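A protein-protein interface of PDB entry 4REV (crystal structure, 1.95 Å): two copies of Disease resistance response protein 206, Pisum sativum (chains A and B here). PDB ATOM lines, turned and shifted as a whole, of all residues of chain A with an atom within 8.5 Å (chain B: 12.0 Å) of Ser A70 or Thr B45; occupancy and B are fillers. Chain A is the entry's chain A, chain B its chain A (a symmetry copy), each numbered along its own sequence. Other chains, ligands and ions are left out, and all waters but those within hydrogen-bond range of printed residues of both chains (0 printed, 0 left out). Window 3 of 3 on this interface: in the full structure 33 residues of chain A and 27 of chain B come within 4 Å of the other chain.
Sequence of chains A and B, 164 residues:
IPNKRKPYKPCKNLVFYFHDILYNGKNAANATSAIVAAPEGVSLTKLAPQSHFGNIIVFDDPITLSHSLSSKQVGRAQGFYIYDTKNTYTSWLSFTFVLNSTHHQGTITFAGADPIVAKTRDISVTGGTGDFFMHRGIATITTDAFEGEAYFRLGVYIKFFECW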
ATOM      1  N   TYR A  17       6.428   0.621  -1.577  1.00  0.00           N
ATOM      2  CA  TYR A  17       7.403   1.468  -2.274  1.00  0.00           C
ATOM      3  C   TYR A  17       6.666   2.502  -3.093  1.00  0.00           C
ATOM      4  O   TYR A  17       5.634   2.183  -3.696  1.00  0.00           O
ATOM      5  CB  TYR A  17       8.302   0.613  -3.167  1.00  0.00           C
ATOM      6  CG  TYR A  17       9.079  -0.375  -2.349  1.00  0.00           C
ATOM      7  CD1 TYR A  17       8.515  -1.588  -1.989  1.00  0.00           C
ATOM      8  CD2 TYR A  17      10.353  -0.076  -1.892  1.00  0.00           C
ATOM      9  CE1 TYR A  17       9.198  -2.489  -1.214  1.00  0.00           C
ATOM     10  CE2 TYR A  17      11.050  -0.971  -1.106  1.00  0.00           C
ATOM     11  CZ  TYR A  17      10.466  -2.177  -0.776  1.00  0.00           C
ATOM     12  OH  TYR A  17      11.144  -3.078   0.000  1.00  0.00           O
ATOM     13  N   HIS A  19       7.359   5.860  -6.054  1.00  0.00           N
ATOM     14  CA  HIS A  19       8.322   6.202  -7.079  1.00  0.00           C
ATOM     15  C   HIS A  19       8.147   7.640  -7.498  1.00  0.00           C
ATOM     16  O   HIS A  19       7.086   8.030  -7.958  1.00  0.00           O
ATOM     17  CB  HIS A  19       8.157   5.278  -8.287  1.00  0.00           C
ATOM     18  CG  HIS A  19       8.186   3.822  -7.944  1.00  0.00           C
ATOM     19  ND1 HIS A  19       9.286   3.028  -8.170  1.00  0.00           N
ATOM     20  CD2 HIS A  19       7.238   3.018  -7.412  1.00  0.00           C
ATOM     21  CE1 HIS A  19       9.023   1.794  -7.781  1.00  0.00           C
ATOM     22  NE2 HIS A  19       7.788   1.762  -7.307  1.00  0.00           N
ATOM     23  N   ASP A  60       2.276  13.114  -7.164  1.00  0.00           N
ATOM     24  CA  ASP A  60       1.251  12.076  -7.216  1.00  0.00           C
ATOM     25  C   ASP A  60       1.944  10.853  -7.783  1.00  0.00           C
ATOM     26  O   ASP A  60       2.160  10.766  -8.984  1.00  0.00           O
ATOM     27  CB  ASP A  60       0.057  12.515  -8.076  1.00  0.00           C
ATOM     28  CG  ASP A  60      -0.970  11.399  -8.296  1.00  0.00           C
ATOM     29  OD1 ASP A  60      -0.908  10.342  -7.627  1.00  0.00           O
ATOM     30  OD2 ASP A  60      -1.877  11.599  -9.124  1.00  0.00           O
ATOM     31  N   ASP A  61       2.336   9.938  -6.902  1.00  0.00           N
ATOM     32  CA  ASP A  61       3.246   8.866  -7.277  1.00  0.00           C
ATOM     33  C   ASP A  61       2.631   7.490  -7.083  1.00  0.00           C
ATOM     34  O   ASP A  61       1.906   7.259  -6.119  1.00  0.00           O
ATOM     35  CB  ASP A  61       4.531   8.949  -6.459  1.00  0.00           C
ATOM     36  CG  ASP A  61       5.373  10.166  -6.795  1.00  0.00           C
ATOM     37  OD1 ASP A  61       5.222  10.751  -7.898  1.00  0.00           O
ATOM     38  OD2 ASP A  61       6.218  10.506  -5.946  1.00  0.00           O
ATOM     39  N   PRO A  62       2.936   6.564  -7.999  1.00  0.00           N
ATOM     40  CA  PRO A  62       2.444   5.198  -7.824  1.00  0.00           C
ATOM     41  C   PRO A  62       3.079   4.514  -6.614  1.00  0.00           C
ATOM     42  O   PRO A  62       4.289   4.617  -6.386  1.00  0.00           O
ATOM     43  CB  PRO A  62       2.855   4.506  -9.136  1.00  0.00           C
ATOM     44  CG  PRO A  62       4.065   5.251  -9.574  1.00  0.00           C
ATOM     45  CD  PRO A  62       3.800   6.691  -9.187  1.00  0.00           C
ATOM     46  N   ILE A  63       2.245   3.826  -5.846  1.00  0.00           N
ATOM     47  CA  ILE A  63       2.702   2.922  -4.799  1.00  0.00           C
ATOM     48  C   ILE A  63       2.665   1.467  -5.269  1.00  0.00           C
ATOM     49  O   ILE A  63       1.637   0.996  -5.755  1.00  0.00           O
ATOM     50  CB  ILE A  63       1.835   3.054  -3.549  1.00  0.00           C
ATOM     51  CG1 ILE A  63       1.824   4.499  -3.066  1.00  0.00           C
ATOM     52  CG2 ILE A  63       2.318   2.110  -2.459  1.00  0.00           C
ATOM     53  CD1 ILE A  63       0.737   4.766  -1.985  1.00  0.00           C
ATOM     54  N   THR A  64       3.774   0.753  -5.111  1.00  0.00           N
ATOM     55  CA  THR A  64       3.838  -0.640  -5.522  1.00  0.00           C
ATOM     56  C   THR A  64       4.133  -1.583  -4.347  1.00  0.00           C
ATOM     57  O   THR A  64       4.601  -1.147  -3.292  1.00  0.00           O
ATOM     58  CB  THR A  64       4.900  -0.827  -6.620  1.00  0.00           C
ATOM     59  OG1 THR A  64       6.185  -0.443  -6.116  1.00  0.00           O
ATOM     60  CG2 THR A  64       4.554   0.029  -7.847  1.00  0.00           C
ATOM     61  N   LEU A  65       3.840  -2.867  -4.532  1.00  0.00           N
ATOM     62  CA  LEU A  65       4.095  -3.883  -3.504  1.00  0.00           C
ATOM     63  C   LEU A  65       5.584  -4.153  -3.345  1.00  0.00           C
ATOM     64  O   LEU A  65       6.072  -4.393  -2.243  1.00  0.00           O
ATOM     65  CB  LEU A  65       3.386  -5.200  -3.839  1.00  0.00           C
ATOM     66  CG  LEU A  65       1.885  -5.297  -3.574  1.00  0.00           C
ATOM     67  CD1 LEU A  65       1.367  -6.651  -4.030  1.00  0.00           C
ATOM     68  CD2 LEU A  65       1.563  -5.052  -2.098  1.00  0.00           C
ATOM     69  N   SER A  66       6.303  -4.131  -4.456  1.00  0.00           N
ATOM     70  CA  SER A  66       7.727  -4.408  -4.414  1.00  0.00           C
ATOM     71  C   SER A  66       8.534  -3.300  -5.077  1.00  0.00           C
ATOM     72  O   SER A  66       8.004  -2.226  -5.392  1.00  0.00           O
ATOM     73  CB  SER A  66       8.029  -5.762  -5.065  1.00  0.00           C
ATOM     74  OG  SER A  66       7.653  -5.780  -6.428  1.00  0.00           O
ATOM     75  N   HIS A  67       9.822  -3.562  -5.262  1.00  0.00           N
ATOM     76  CA  HIS A  67      10.760  -2.524  -5.673  1.00  0.00           C
ATOM     77  C   HIS A  67      10.507  -1.988  -7.080  1.00  0.00           C
ATOM     78  O   HIS A  67      10.566  -0.783  -7.303  1.00  0.00           O
ATOM     79  CB  HIS A  67      12.199  -3.046  -5.563  1.00  0.00           C
ATOM     80  CG  HIS A  67      12.563  -3.482  -4.179  1.00  0.00           C
ATOM     81  ND1 HIS A  67      12.322  -4.756  -3.711  1.00  0.00           N
ATOM     82  CD2 HIS A  67      13.089  -2.791  -3.139  1.00  0.00           C
ATOM     83  CE1 HIS A  67      12.720  -4.841  -2.453  1.00  0.00           C
ATOM     84  NE2 HIS A  67      13.182  -3.660  -2.081  1.00  0.00           N
ATOM     85  N   SER A  68      10.216  -2.874  -8.022  1.00  0.00           N
ATOM     86  CA  SER A  68      10.063  -2.456  -9.407  1.00  0.00           C
ATOM     87  C   SER A  68       8.822  -1.607  -9.635  1.00  0.00           C
ATOM     88  O   SER A  68       7.754  -1.872  -9.079  1.00  0.00           O
ATOM     89  CB  SER A  68      10.024  -3.667 -10.335  1.00  0.00           C
ATOM     90  OG  SER A  68       9.507  -3.287 -11.598  1.00  0.00           O
ATOM     91  N   LEU A  69       8.985  -0.587 -10.470  1.00  0.00           N
ATOM     92  CA  LEU A  69       7.905   0.300 -10.873  1.00  0.00           C
ATOM     93  C   LEU A  69       6.780  -0.457 -11.587  1.00  0.00           C
ATOM     94  O   LEU A  69       5.635  -0.009 -11.603  1.00  0.00           O
ATOM     95  CB  LEU A  69       8.461   1.408 -11.781  1.00  0.00           C
ATOM     96  CG  LEU A  69       7.549   2.426 -12.475  1.00  0.00           C
ATOM     97  CD1 LEU A  69       8.302   3.730 -12.688  1.00  0.00           C
ATOM     98  CD2 LEU A  69       7.045   1.910 -13.810  1.00  0.00           C
ATOM     99  N   SER A  70       7.101  -1.599 -12.179  1.00  0.00           N
ATOM    100  CA  SER A  70       6.102  -2.309 -12.963  1.00  0.00           C
ATOM    101  C   SER A  70       5.464  -3.439 -12.166  1.00  0.00           C
ATOM    102  O   SER A  70       4.750  -4.268 -12.729  1.00  0.00           O
ATOM    103  CB  SER A  70       6.718  -2.845 -14.262  1.00  0.00           C
ATOM    104  OG  SER A  70       7.703  -3.826 -13.994  1.00  0.00           O
ATOM    105  N   SER A  71       5.711  -3.470 -10.855  1.00  0.00           N
ATOM    106  CA  SER A  71       5.050  -4.444  -9.984  1.00  0.00           C
ATOM    107  C   SER A  71       3.670  -3.903  -9.643  1.00  0.00           C
ATOM    108  O   SER A  71       3.403  -2.738  -9.903  1.00  0.00           O
ATOM    109  CB  SER A  71       5.851  -4.699  -8.709  1.00  0.00           C
ATOM    110  OG  SER A  71       6.088  -3.494  -7.986  1.00  0.00           O
ATOM    111  N   LYS A  72       2.806  -4.727  -9.046  1.00  0.00           N
ATOM    112  CA  LYS A  72       1.409  -4.344  -8.852  1.00  0.00           C
ATOM    113  C   LYS A  72       1.294  -3.035  -8.077  1.00  0.00           C
ATOM    114  O   LYS A  72       1.886  -2.867  -7.025  1.00  0.00           O
ATOM    115  CB  LYS A  72       0.618  -5.432  -8.124  1.00  0.00           C
ATOM    116  CG  LYS A  72      -0.891  -5.316  -8.359  1.00  0.00           C
ATOM    117  CD  LYS A  72      -1.731  -5.839  -7.190  1.00  0.00           C
ATOM    118  CE  LYS A  72      -2.781  -4.814  -6.735  1.00  0.00           C
ATOM    119  NZ  LYS A  72      -3.948  -5.448  -6.046  1.00  0.00           N
ATOM    120  N   GLN A  73       0.545  -2.089  -8.614  1.00  0.00           N
ATOM    121  CA  GLN A  73       0.279  -0.859  -7.889  1.00  0.00           C
ATOM    122  C   GLN A  73      -0.905  -1.014  -6.964  1.00  0.00           C
ATOM    123  O   GLN A  73      -1.928  -1.591  -7.348  1.00  0.00           O
ATOM    124  CB  GLN A  73      -0.007   0.285  -8.840  1.00  0.00           C
ATOM    125  CG  GLN A  73      -0.487   1.533  -8.119  1.00  0.00           C
ATOM    126  CD  GLN A  73      -0.918   2.614  -9.096  1.00  0.00           C
ATOM    127  OE1 GLN A  73      -0.091   3.252  -9.744  1.00  0.00           O
ATOM    128  NE2 GLN A  73      -2.228   2.785  -9.221  1.00  0.00           N
ATOM    129  N   VAL A  74      -0.776  -0.454  -5.768  1.00  0.00           N
ATOM    130  CA  VAL A  74      -1.777  -0.633  -4.739  1.00  0.00           C
ATOM    131  C   VAL A  74      -2.376   0.708  -4.309  1.00  0.00           C
ATOM    132  O   VAL A  74      -3.275   0.741  -3.486  1.00  0.00           O
ATOM    133  CB  VAL A  74      -1.187  -1.362  -3.527  1.00  0.00           C
ATOM    134  CG1 VAL A  74      -0.887  -2.805  -3.902  1.00  0.00           C
ATOM    135  CG2 VAL A  74       0.081  -0.661  -3.042  1.00  0.00           C
ATOM    136  N   GLY A  75      -1.906   1.797  -4.909  1.00  0.00           N
ATOM    137  CA  GLY A  75      -2.431   3.120  -4.622  1.00  0.00           C
ATOM    138  C   GLY A  75      -1.537   4.232  -5.151  1.00  0.00           C
ATOM    139  O   GLY A  75      -0.669   3.991  -5.994  1.00  0.00           O
ATOM    140  N   ARG A  76      -1.775   5.448  -4.668  1.00  0.00           N
ATOM    141  CA  ARG A  76      -0.993   6.617  -5.034  1.00  0.00           C
ATOM    142  C   ARG A  76      -0.503   7.329  -3.783  1.00  0.00           C
ATOM    143  O   ARG A  76      -1.247   7.457  -2.788  1.00  0.00           O
ATOM    144  CB  ARG A  76      -1.817   7.610  -5.869  1.00  0.00           C
ATOM    145  CG  ARG A  76      -2.431   7.055  -7.164  1.00  0.00           C
ATOM    146  CD  ARG A  76      -1.394   6.549  -8.164  1.00  0.00           C
ATOM    147  NE  ARG A  76      -0.611   7.639  -8.749  1.00  0.00           N
ATOM    148  CZ  ARG A  76       0.185   7.496  -9.802  1.00  0.00           C
ATOM    149  NH1 ARG A  76       0.288   6.312 -10.397  1.00  0.00           N
ATOM    150  NH2 ARG A  76       0.870   8.534 -10.270  1.00  0.00           N
ATOM    151  N   TYR A 151      15.089   9.904 -10.843  1.00  0.00           N
ATOM    152  CA  TYR A 151      14.291   8.829 -10.264  1.00  0.00           C
ATOM    153  C   TYR A 151      14.654   8.494  -8.809  1.00  0.00           C
ATOM    154  O   TYR A 151      15.794   8.119  -8.510  1.00  0.00           O
ATOM    155  CB  TYR A 151      14.419   7.565 -11.121  1.00  0.00           C
ATOM    156  CG  TYR A 151      13.675   6.387 -10.536  1.00  0.00           C
ATOM    157  CD1 TYR A 151      12.290   6.345 -10.552  1.00  0.00           C
ATOM    158  CD2 TYR A 151      14.358   5.331  -9.946  1.00  0.00           C
ATOM    159  CE1 TYR A 151      11.601   5.277 -10.009  1.00  0.00           C
ATOM    160  CE2 TYR A 151      13.679   4.258  -9.395  1.00  0.00           C
ATOM    161  CZ  TYR A 151      12.299   4.235  -9.434  1.00  0.00           C
ATOM    162  OH  TYR A 151      11.611   3.173  -8.894  1.00  0.00           O
ATOM    163  N   THR B  45       3.699   1.766 -12.809  1.00  0.00           N
ATOM    164  CA  THR B  45       2.329   1.330 -13.069  1.00  0.00           C
ATOM    165  C   THR B  45       1.295   2.443 -13.206  1.00  0.00           C
ATOM    166  O   THR B  45       1.437   3.506 -12.603  1.00  0.00           O
ATOM    167  CB  THR B  45       1.855   0.406 -11.974  1.00  0.00           C
ATOM    168  OG1 THR B  45       2.056   1.062 -10.720  1.00  0.00           O
ATOM    169  CG2 THR B  45       2.619  -0.883 -12.013  1.00  0.00           C
ATOM    170  N   LYS B  46       0.230   2.119 -13.949  1.00  0.00           N
ATOM    171  CA  LYS B  46      -0.833   3.018 -14.413  1.00  0.00           C
ATOM    172  C   LYS B  46      -0.083   4.323 -14.762  1.00  0.00           C
ATOM    173  O   LYS B  46       0.906   4.285 -15.488  1.00  0.00           O
ATOM    174  CB  LYS B  46      -1.989   3.135 -13.347  1.00  0.00           C
ATOM    175  CG  LYS B  46      -2.844   4.442 -13.219  1.00  0.00           C
ATOM    176  CD  LYS B  46      -3.844   4.565 -12.052  1.00  0.00           C
ATOM    177  CE  LYS B  46      -3.241   4.996 -10.738  1.00  0.00           C
ATOM    178  NZ  LYS B  46      -4.177   4.861  -9.573  1.00  0.00           N
ATOM    179  N   LEU B  47      -0.529   5.451 -14.235  1.00  0.00           N
ATOM    180  CA  LEU B  47       0.091   6.749 -14.386  1.00  0.00           C
ATOM    181  C   LEU B  47       1.509   6.745 -13.818  1.00  0.00           C
ATOM    182  O   LEU B  47       1.753   6.191 -12.751  1.00  0.00           O
ATOM    183  CB  LEU B  47      -0.786   7.790 -13.687  1.00  0.00           C
ATOM    184  CG  LEU B  47      -0.769   9.263 -14.094  1.00  0.00           C
ATOM    185  CD1 LEU B  47      -1.281   9.466 -15.523  1.00  0.00           C
ATOM    186  CD2 LEU B  47      -1.623  10.038 -13.096  1.00  0.00           C
ATOM    187  N   ALA B  48       2.442   7.341 -14.550  1.00  0.00           N
ATOM    188  CA  ALA B  48       3.818   7.486 -14.090  1.00  0.00           C
ATOM    189  C   ALA B  48       3.851   8.450 -12.898  1.00  0.00           C
ATOM    190  O   ALA B  48       2.842   9.099 -12.615  1.00  0.00           O
ATOM    191  CB  ALA B  48       4.712   7.982 -15.245  1.00  0.00           C
ATOM    192  N   PRO B  49       4.992   8.524 -12.174  1.00  0.00           N
ATOM    193  CA  PRO B  49       5.127   9.497 -11.075  1.00  0.00           C
ATOM    194  C   PRO B  49       4.918  10.872 -11.610  1.00  0.00           C
ATOM    195  O   PRO B  49       5.318  11.163 -12.730  1.00  0.00           O
ATOM    196  CB  PRO B  49       6.574   9.358 -10.632  1.00  0.00           C
ATOM    197  CG  PRO B  49       6.967   8.028 -11.047  1.00  0.00           C
ATOM    198  CD  PRO B  49       6.198   7.693 -12.290  1.00  0.00           C
ATOM    199  N   GLN B  50       4.315  11.743 -10.847  1.00  0.00           N
ATOM    200  CA  GLN B  50       3.913  12.927 -11.515  1.00  0.00           C
ATOM    201  C   GLN B  50       4.307  13.992 -10.462  1.00  0.00           C
ATOM    202  O   GLN B  50       3.980  13.831  -9.305  1.00  0.00           O
ATOM    203  CB  GLN B  50       2.421  12.945 -11.779  1.00  0.00           C
ATOM    204  CG  GLN B  50       1.954  12.707 -13.226  1.00  0.00           C
ATOM    205  CD  GLN B  50       0.471  13.080 -13.299  1.00  0.00           C
ATOM    206  OE1 GLN B  50       0.141  13.950 -14.141  1.00  0.00           O
ATOM    207  NE2 GLN B  50      -0.310  12.750 -12.206  1.00  0.00           N
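O of His A19 touches CB of Pro B49, at 3.0 Å. Asp A60 touches Pro B49. Pro B49 touches Asp A61. CB of Pro A62 touches OG1 of Thr B45 (3.9 Å). Pro B49 touches Pro A62. CG2 of Thr A64 touches OG1 of Thr B45 (3.9 Å). C of Ser A70 touches CG2 of Thr B45, at 3.8 Å. Ser A71 touches Thr B45. NH1 of Arg A76 touches O of Thr B45, at 3.7 Å. CD of Arg A76 touches CE of Lys B46 (3.5 Å).
Hydrophobic or aromatic side chains of chain B that line the printed part of chain A: Leu B47 and Pro B49. Printed residues of chain A that touch a printed residue of chain B: His A19, Asp A60, Asp A61, Pro A62, Thr A64, Leu A69, Ser A70, Ser A71, Gln A73 and Arg A76. Hydrophobic or aromatic side chains of chain A within 4 Å of the printed part of chain B: Pro A62 and Leu A69.
The backbone carbonyl oxygen (O) of Tyr A17 is in hydrogen-bond range of the backbone NH (N) of Thr A64, 2.7 Å away. N of His A19 lies within hydrogen-bond range of O of Pro A62 (3.3 Å). The side-chain carboxylate of Asp A60 is in salt-bridge range of the guanidinium group of Arg A76. The side-chain hydroxyl of Thr A64 lies within hydrogen-bond range of the backbone carbonyl oxygen of Ser A66, at 2.6 Å. The backbone NH (N) of Ser A70 sits at hydrogen-bond distance from the side-chain hydroxyl (OG) of Ser A68 (3.0 Å). O of Ser A68 lies within hydrogen-bond range of OG of Ser A71, 2.6 Å away.
No position is printed for both chains. Of the 17 pairs that touch across the chains among the printed residues, none has its exchanged pair printed and touching as well.
The backbone carbonyl oxygen (O) of Gln B50 is in hydrogen-bond range of the backbone NH (N) of Asp A60, 2.8 Å away. OD1 of Asp A61 is in hydrogen-bond range of N of Gln B50, at 3.2 Å. The backbone carbonyl oxygen (O) of Leu A69 lies within hydrogen-bond range of the backbone NH (N) of Thr B45 (2.9 Å). OE1 of Gln A73 sits close to OG1 of Thr B45, 3.2 Å away. NZ of Lys B46 lies close to NE2 of Gln A73, 2.9 Å away. NH1 of Arg A76 sits at hydrogen-bond distance from O of Leu B47 (2.8 Å). NH2 of Arg A76 is in hydrogen-bond range of O of Ala B48 (3.1 Å).
Pro A62 touches just these residues of chain B: Thr B45 (3.9 Å) and Pro B49 (3.6 Å). Leu A65 touches none of the printed residues of chain B. Of chain B, only Thr B45 comes within 4 Å of Leu A69. Ser A70 touches just one residue of chain B: Thr B45 (3.8 Å). Lys A72 touches none of the printed residues of chain B. Gln A73 touches just these residues of chain B: Thr B45 (2.9 Å) and Lys B46 (2.9 Å). No residue of chain B comes within 4 Å of Gly A75. Printed residues of chain B within 4 Å of Arg A76: Thr B45 (3.7 Å), Lys B46 (3.5 Å), Leu B47 (2.8 Å) and Ala B48 (3.1 Å). Printed residues of chain A within 4 Å of Gln B50: Asp A60 (2.8 Å) and Asp A61 (3.2 Å). The nearest residue of chain B that does not touch Ser A70 is Lys B46 (7.4 Å). The nearest residue of chain A that does not touch Thr B45 is Lys A72 (4.7 Å).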
